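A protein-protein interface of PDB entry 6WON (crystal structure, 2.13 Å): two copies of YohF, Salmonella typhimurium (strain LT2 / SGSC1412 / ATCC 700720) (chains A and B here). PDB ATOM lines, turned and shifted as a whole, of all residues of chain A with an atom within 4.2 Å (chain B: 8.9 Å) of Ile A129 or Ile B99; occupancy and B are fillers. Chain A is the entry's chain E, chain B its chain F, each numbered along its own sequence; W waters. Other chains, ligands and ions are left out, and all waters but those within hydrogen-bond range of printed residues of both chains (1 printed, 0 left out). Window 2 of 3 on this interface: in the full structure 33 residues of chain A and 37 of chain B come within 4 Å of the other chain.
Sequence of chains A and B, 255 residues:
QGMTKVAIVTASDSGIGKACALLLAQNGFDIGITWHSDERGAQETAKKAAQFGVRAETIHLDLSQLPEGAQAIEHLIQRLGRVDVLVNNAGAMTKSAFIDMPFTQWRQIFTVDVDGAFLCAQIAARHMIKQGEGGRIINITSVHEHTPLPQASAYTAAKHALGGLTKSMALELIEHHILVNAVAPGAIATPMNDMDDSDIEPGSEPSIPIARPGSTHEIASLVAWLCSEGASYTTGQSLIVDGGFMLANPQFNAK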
ATOM      1  N   GLN A 122      30.841  -0.501 -20.437  1.00  0.00           N
ATOM      2  CA  GLN A 122      31.125  -1.490 -21.476  1.00  0.00           C
ATOM      3  C   GLN A 122      30.857  -2.899 -20.974  1.00  0.00           C
ATOM      4  O   GLN A 122      30.175  -3.694 -21.633  1.00  0.00           O
ATOM      5  CB  GLN A 122      32.576  -1.369 -21.933  1.00  0.00           C
ATOM      6  CG  GLN A 122      32.808  -0.470 -23.129  1.00  0.00           C
ATOM      7  CD  GLN A 122      34.246  -0.535 -23.620  1.00  0.00           C
ATOM      8  OE1 GLN A 122      35.172  -0.833 -22.847  1.00  0.00           O
ATOM      9  NE2 GLN A 122      34.441  -0.269 -24.906  1.00  0.00           N
ATOM     10  N   ALA A 125      27.103  -3.379 -20.304  1.00  0.00           N
ATOM     11  CA  ALA A 125      26.326  -3.378 -21.542  1.00  0.00           C
ATOM     12  C   ALA A 125      26.559  -4.646 -22.353  1.00  0.00           C
ATOM     13  O   ALA A 125      25.649  -5.119 -23.045  1.00  0.00           O
ATOM     14  CB  ALA A 125      26.665  -2.151 -22.385  1.00  0.00           C
ATOM     15  N   ARG A 126      27.761  -5.216 -22.272  1.00  0.00           N
ATOM     16  CA  ARG A 126      28.030  -6.462 -22.980  1.00  0.00           C
ATOM     17  C   ARG A 126      27.138  -7.580 -22.461  1.00  0.00           C
ATOM     18  O   ARG A 126      26.536  -8.326 -23.247  1.00  0.00           O
ATOM     19  CB  ARG A 126      29.508  -6.835 -22.841  1.00  0.00           C
ATOM     20  CG  ARG A 126      30.410  -6.086 -23.815  1.00  0.00           C
ATOM     21  CD  ARG A 126      31.871  -6.057 -23.357  1.00  0.00           C
ATOM     22  NE  ARG A 126      32.636  -5.050 -24.086  1.00  0.00           N
ATOM     23  CZ  ARG A 126      33.895  -4.715 -23.815  1.00  0.00           C
ATOM     24  NH1 ARG A 126      34.551  -5.315 -22.826  1.00  0.00           N
ATOM     25  NH2 ARG A 126      34.502  -3.779 -24.540  1.00  0.00           N
ATOM     26  N   HIS A 127      27.037  -7.711 -21.133  1.00  0.00           N
ATOM     27  CA  HIS A 127      26.165  -8.736 -20.565  1.00  0.00           C
ATOM     28  C   HIS A 127      24.703  -8.448 -20.896  1.00  0.00           C
ATOM     29  O   HIS A 127      23.942  -9.362 -21.238  1.00  0.00           O
ATOM     30  CB  HIS A 127      26.377  -8.832 -19.052  1.00  0.00           C
ATOM     31  CG  HIS A 127      27.653  -9.517 -18.659  1.00  0.00           C
ATOM     32  ND1 HIS A 127      27.701 -10.837 -18.264  1.00  0.00           N
ATOM     33  CD2 HIS A 127      28.927  -9.061 -18.599  1.00  0.00           C
ATOM     34  CE1 HIS A 127      28.951 -11.167 -17.981  1.00  0.00           C
ATOM     35  NE2 HIS A 127      29.715 -10.108 -18.178  1.00  0.00           N
ATOM     36  N   MET A 128      24.293  -7.179 -20.811  1.00  0.00           N
ATOM     37  CA  MET A 128      22.914  -6.835 -21.139  1.00  0.00           C
ATOM     38  C   MET A 128      22.569  -7.245 -22.564  1.00  0.00           C
ATOM     39  O   MET A 128      21.468  -7.750 -22.827  1.00  0.00           O
ATOM     40  CB  MET A 128      22.688  -5.339 -20.948  1.00  0.00           C
ATOM     41  CG  MET A 128      22.681  -4.887 -19.498  1.00  0.00           C
ATOM     42  SD  MET A 128      22.691  -3.092 -19.384  1.00  0.00           S
ATOM     43  CE  MET A 128      22.546  -2.880 -17.605  1.00  0.00           C
ATOM     44  N   ILE A 129      23.494  -7.032 -23.499  1.00  0.00           N
ATOM     45  CA  ILE A 129      23.242  -7.393 -24.890  1.00  0.00           C
ATOM     46  C   ILE A 129      23.079  -8.901 -25.020  1.00  0.00           C
ATOM     47  O   ILE A 129      22.123  -9.391 -25.633  1.00  0.00           O
ATOM     48  CB  ILE A 129      24.368  -6.861 -25.796  1.00  0.00           C
ATOM     49  CG1 ILE A 129      24.254  -5.337 -25.928  1.00  0.00           C
ATOM     50  CG2 ILE A 129      24.304  -7.537 -27.164  1.00  0.00           C
ATOM     51  CD1 ILE A 129      25.462  -4.676 -26.562  1.00  0.00           C
ATOM     52  N   LYS A 130      23.999  -9.662 -24.420  1.00  0.00           N
ATOM     53  CA  LYS A 130      23.940 -11.118 -24.527  1.00  0.00           C
ATOM     54  C   LYS A 130      22.676 -11.691 -23.889  1.00  0.00           C
ATOM     55  O   LYS A 130      22.061 -12.609 -24.444  1.00  0.00           O
ATOM     56  CB  LYS A 130      25.184 -11.746 -23.902  1.00  0.00           C
ATOM     57  CG  LYS A 130      25.180 -13.269 -23.989  1.00  0.00           C
ATOM     58  CD  LYS A 130      26.390 -13.829 -24.723  1.00  0.00           C
ATOM     59  CE  LYS A 130      26.439 -15.352 -24.631  1.00  0.00           C
ATOM     60  NZ  LYS A 130      26.874 -15.831 -23.278  1.00  0.00           N
ATOM     61  N   GLN A 131      22.285 -11.179 -22.714  1.00  0.00           N
ATOM     62  CA  GLN A 131      21.045 -11.626 -22.075  1.00  0.00           C
ATOM     63  C   GLN A 131      19.835 -11.398 -22.971  1.00  0.00           C
ATOM     64  O   GLN A 131      18.905 -12.211 -22.973  1.00  0.00           O
ATOM     65  CB  GLN A 131      20.830 -10.911 -20.737  1.00  0.00           C
ATOM     66  CG  GLN A 131      21.878 -11.201 -19.670  1.00  0.00           C
ATOM     67  CD  GLN A 131      22.063 -10.037 -18.695  1.00  0.00           C
ATOM     68  OE1 GLN A 131      23.002 -10.026 -17.902  1.00  0.00           O
ATOM     69  NE2 GLN A 131      21.154  -9.062 -18.745  1.00  0.00           N
ATOM     70  N   GLY A 132      19.824 -10.303 -23.730  1.00  0.00           N
ATOM     71  CA  GLY A 132      18.742 -10.045 -24.655  1.00  0.00           C
ATOM     72  C   GLY A 132      17.468  -9.528 -24.030  1.00  0.00           C
ATOM     73  O   GLY A 132      16.406  -9.620 -24.655  1.00  0.00           O
ATOM     74  N   HIS A 176      19.518  -2.266 -28.465  1.00  0.00           N
ATOM     75  CA  HIS A 176      19.503  -3.400 -27.553  1.00  0.00           C
ATOM     76  C   HIS A 176      18.560  -3.203 -26.370  1.00  0.00           C
ATOM     77  O   HIS A 176      18.627  -3.974 -25.409  1.00  0.00           O
ATOM     78  CB  HIS A 176      20.916  -3.673 -27.048  1.00  0.00           C
ATOM     79  CG  HIS A 176      21.902  -3.905 -28.145  1.00  0.00           C
ATOM     80  ND1 HIS A 176      21.861  -5.020 -28.954  1.00  0.00           N
ATOM     81  CD2 HIS A 176      22.951  -3.163 -28.574  1.00  0.00           C
ATOM     82  CE1 HIS A 176      22.847  -4.960 -29.830  1.00  0.00           C
ATOM     83  NE2 HIS A 176      23.526  -3.845 -29.619  1.00  0.00           N
ATOM     84  N   ILE A 178      18.637  -0.974 -24.130  1.00  0.00           N
ATOM     85  CA  ILE A 178      19.361  -0.455 -22.982  1.00  0.00           C
ATOM     86  C   ILE A 178      19.194   1.054 -22.995  1.00  0.00           C
ATOM     87  O   ILE A 178      19.646   1.727 -23.931  1.00  0.00           O
ATOM     88  CB  ILE A 178      20.843  -0.853 -23.017  1.00  0.00           C
ATOM     89  CG1 ILE A 178      20.992  -2.376 -22.899  1.00  0.00           C
ATOM     90  CG2 ILE A 178      21.618  -0.115 -21.915  1.00  0.00           C
ATOM     91  CD1 ILE A 178      22.284  -2.899 -23.512  1.00  0.00           C
ATOM     92  N   SER B  96      34.810   4.743 -33.608  1.00  0.00           N
ATOM     93  CA  SER B  96      34.884   3.416 -33.014  1.00  0.00           C
ATOM     94  C   SER B  96      33.626   3.159 -32.194  1.00  0.00           C
ATOM     95  O   SER B  96      33.205   4.022 -31.418  1.00  0.00           O
ATOM     96  CB  SER B  96      36.133   3.287 -32.142  1.00  0.00           C
ATOM     97  OG  SER B  96      36.013   2.203 -31.243  1.00  0.00           O
ATOM     98  N   ALA B  97      33.017   1.986 -32.359  1.00  0.00           N
ATOM     99  CA  ALA B  97      31.798   1.652 -31.625  1.00  0.00           C
ATOM    100  C   ALA B  97      32.059   1.589 -30.124  1.00  0.00           C
ATOM    101  O   ALA B  97      33.055   1.016 -29.674  1.00  0.00           O
ATOM    102  CB  ALA B  97      31.248   0.308 -32.108  1.00  0.00           C
ATOM    103  N   PHE B  98      31.125   2.141 -29.340  1.00  0.00           N
ATOM    104  CA  PHE B  98      31.318   2.191 -27.891  1.00  0.00           C
ATOM    105  C   PHE B  98      31.514   0.801 -27.296  1.00  0.00           C
ATOM    106  O   PHE B  98      32.387   0.599 -26.438  1.00  0.00           O
ATOM    107  CB  PHE B  98      30.133   2.883 -27.210  1.00  0.00           C
ATOM    108  CG  PHE B  98      29.918   2.449 -25.782  1.00  0.00           C
ATOM    109  CD1 PHE B  98      30.617   3.045 -24.748  1.00  0.00           C
ATOM    110  CD2 PHE B  98      29.011   1.449 -25.471  1.00  0.00           C
ATOM    111  CE1 PHE B  98      30.411   2.638 -23.424  1.00  0.00           C
ATOM    112  CE2 PHE B  98      28.812   1.035 -24.162  1.00  0.00           C
ATOM    113  CZ  PHE B  98      29.513   1.628 -23.139  1.00  0.00           C
ATOM    114  N   ILE B  99      30.709  -0.169 -27.736  1.00  0.00           N
ATOM    115  CA  ILE B  99      30.627  -1.442 -27.022  1.00  0.00           C
ATOM    116  C   ILE B  99      31.976  -2.161 -26.959  1.00  0.00           C
ATOM    117  O   ILE B  99      32.285  -2.813 -25.952  1.00  0.00           O
ATOM    118  CB  ILE B  99      29.528  -2.324 -27.649  1.00  0.00           C
ATOM    119  CG1 ILE B  99      29.191  -3.507 -26.723  1.00  0.00           C
ATOM    120  CG2 ILE B  99      29.932  -2.802 -29.038  1.00  0.00           C
ATOM    121  CD1 ILE B  99      28.646  -3.099 -25.373  1.00  0.00           C
ATOM    122  N   ASP B 100      32.812  -2.046 -28.000  1.00  0.00           N
ATOM    123  CA  ASP B 100      34.099  -2.744 -28.021  1.00  0.00           C
ATOM    124  C   ASP B 100      35.280  -1.805 -28.236  1.00  0.00           C
ATOM    125  O   ASP B 100      36.380  -2.272 -28.556  1.00  0.00           O
ATOM    126  CB  ASP B 100      34.119  -3.835 -29.095  1.00  0.00           C
ATOM    127  CG  ASP B 100      33.439  -3.395 -30.375  1.00  0.00           C
ATOM    128  OD1 ASP B 100      33.744  -2.279 -30.864  1.00  0.00           O
ATOM    129  OD2 ASP B 100      32.574  -4.158 -30.875  1.00  0.00           O
ATOM    130  N   MET B 101      35.089  -0.503 -28.073  1.00  0.00           N
ATOM    131  CA  MET B 101      36.198   0.415 -28.251  1.00  0.00           C
ATOM    132  C   MET B 101      37.307   0.070 -27.262  1.00  0.00           C
ATOM    133  O   MET B 101      37.055   0.043 -26.051  1.00  0.00           O
ATOM    134  CB  MET B 101      35.770   1.865 -28.058  1.00  0.00           C
ATOM    135  CG  MET B 101      36.946   2.820 -27.943  1.00  0.00           C
ATOM    136  SD  MET B 101      36.460   4.563 -27.955  1.00  0.00           S
ATOM    137  CE  MET B 101      34.852   4.428 -27.160  1.00  0.00           C
ATOM    138  N   PRO B 102      38.523  -0.215 -27.727  1.00  0.00           N
ATOM    139  CA  PRO B 102      39.636  -0.476 -26.800  1.00  0.00           C
ATOM    140  C   PRO B 102      39.919   0.725 -25.903  1.00  0.00           C
ATOM    141  O   PRO B 102      39.709   1.882 -26.285  1.00  0.00           O
ATOM    142  CB  PRO B 102      40.819  -0.756 -27.735  1.00  0.00           C
ATOM    143  CG  PRO B 102      40.195  -1.138 -29.043  1.00  0.00           C
ATOM    144  CD  PRO B 102      38.922  -0.356 -29.137  1.00  0.00           C
ATOM    145  N   PHE B 103      40.404   0.436 -24.691  1.00  0.00           N
ATOM    146  CA  PHE B 103      40.746   1.513 -23.765  1.00  0.00           C
ATOM    147  C   PHE B 103      41.864   2.394 -24.319  1.00  0.00           C
ATOM    148  O   PHE B 103      41.845   3.618 -24.132  1.00  0.00           O
ATOM    149  CB  PHE B 103      41.143   0.932 -22.401  1.00  0.00           C
ATOM    150  CG  PHE B 103      41.276   1.975 -21.322  1.00  0.00           C
ATOM    151  CD1 PHE B 103      40.258   2.895 -21.101  1.00  0.00           C
ATOM    152  CD2 PHE B 103      42.417   2.047 -20.536  1.00  0.00           C
ATOM    153  CE1 PHE B 103      40.375   3.868 -20.113  1.00  0.00           C
ATOM    154  CE2 PHE B 103      42.541   3.019 -19.543  1.00  0.00           C
ATOM    155  CZ  PHE B 103      41.514   3.931 -19.334  1.00  0.00           C
ATOM    156  N   GLN B 151      28.840   6.240 -33.452  1.00  0.00           N
ATOM    157  CA  GLN B 151      30.115   5.528 -33.577  1.00  0.00           C
ATOM    158  C   GLN B 151      31.314   6.395 -33.197  1.00  0.00           C
ATOM    159  O   GLN B 151      32.440   6.120 -33.609  1.00  0.00           O
ATOM    160  CB  GLN B 151      30.302   4.968 -34.995  1.00  0.00           C
ATOM    161  CG  GLN B 151      29.127   4.128 -35.478  1.00  0.00           C
ATOM    162  CD  GLN B 151      28.927   2.900 -34.619  1.00  0.00           C
ATOM    163  OE1 GLN B 151      29.820   2.047 -34.503  1.00  0.00           O
ATOM    164  NE2 GLN B 151      27.743   2.787 -34.021  1.00  0.00           N
ATOM    165  N   SER B 153      31.839   7.806 -29.649  1.00  0.00           N
ATOM    166  CA  SER B 153      31.509   8.160 -28.273  1.00  0.00           C
ATOM    167  C   SER B 153      32.682   8.845 -27.587  1.00  0.00           C
ATOM    168  O   SER B 153      32.490   9.790 -26.811  1.00  0.00           O
ATOM    169  CB  SER B 153      31.077   6.918 -27.495  1.00  0.00           C
ATOM    170  OG  SER B 153      32.037   5.903 -27.616  1.00  0.00           O
HETATM  171  O   HOH W   1      37.749  -1.012 -23.736  1.00  0.00           O
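The side-chain amide nitrogen of Gln A122 sits at hydrogen-bond distance from the backbone carbonyl oxygen of Phe B98 (2.7 Å). The side-chain amide nitrogen (NE2) of Gln A122 is in hydrogen-bond range of the backbone carbonyl oxygen (O) of Ile B99 (3.5 Å). The backbone carbonyl oxygen of Met B101 lies within hydrogen-bond range of the side-chain amide nitrogen of Gln A122 (2.9 Å). O of Ile B99 is in hydrogen-bond range of NH2 of Arg A126.
The guanidinium group (NH2) of Arg A126 sits close to the side-chain amide oxygen (OE1) of Gln A122, 3.5 Å away.
Asp B100 touches Gln A122 (C to NE2, 3.8 Å). Ala A125 touches Ile B99 (CB to CD1, 3.7 Å). Asp B100 touches Arg A126. Ile A129 touches Ile B99 (CD1 to CD1, 3.7 Å).
Ile A129 touches one residue of chain B. Of the printed residues of chain A, Ile B99 touches Gln A122, Ala A125, Arg A126 and Ile A129. Of the printed residues of chain B, Arg A126 touches Ile B99 and Asp B100. Printed residues of chain B within 4 Å of Ala A125: Ile B99 (3.7 Å). Printed residues of chain B within 4 Å of Gln A122: Phe B98 (2.7 Å), Ile B99 (3.5 Å), Asp B100 (3.8 Å) and Met B101 (2.9 Å). Of the printed residues of chain A, Phe B98 touches Gln A122 (2.7 Å). Phe B103 touches none of the printed residues of chain A. The nearest residue of chain B that does not touch Ile A129 is Phe B98 (7.0 Å).
Hydrophobic or aromatic side chains of chain A that line the printed part of chain B: Ala A125 and Ile A129. Hydrophobic or aromatic side chains of chain B that line the printed part of chain A: Phe B98 and Ile B99. Among the printed residues, 8 pairs touch across the chains. Among the printed residues, no Asp or Glu carboxylate lies within 4 Å of a Lys or Arg side-chain nitrogen of the other chain.
No position is printed for both chains.
Water W1 lies within hydrogen-bond range of O of Met B101 (2.6 Å), OE1 of Gln A122 (2.7 Å) and N of Phe B103 (3.2 Å).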
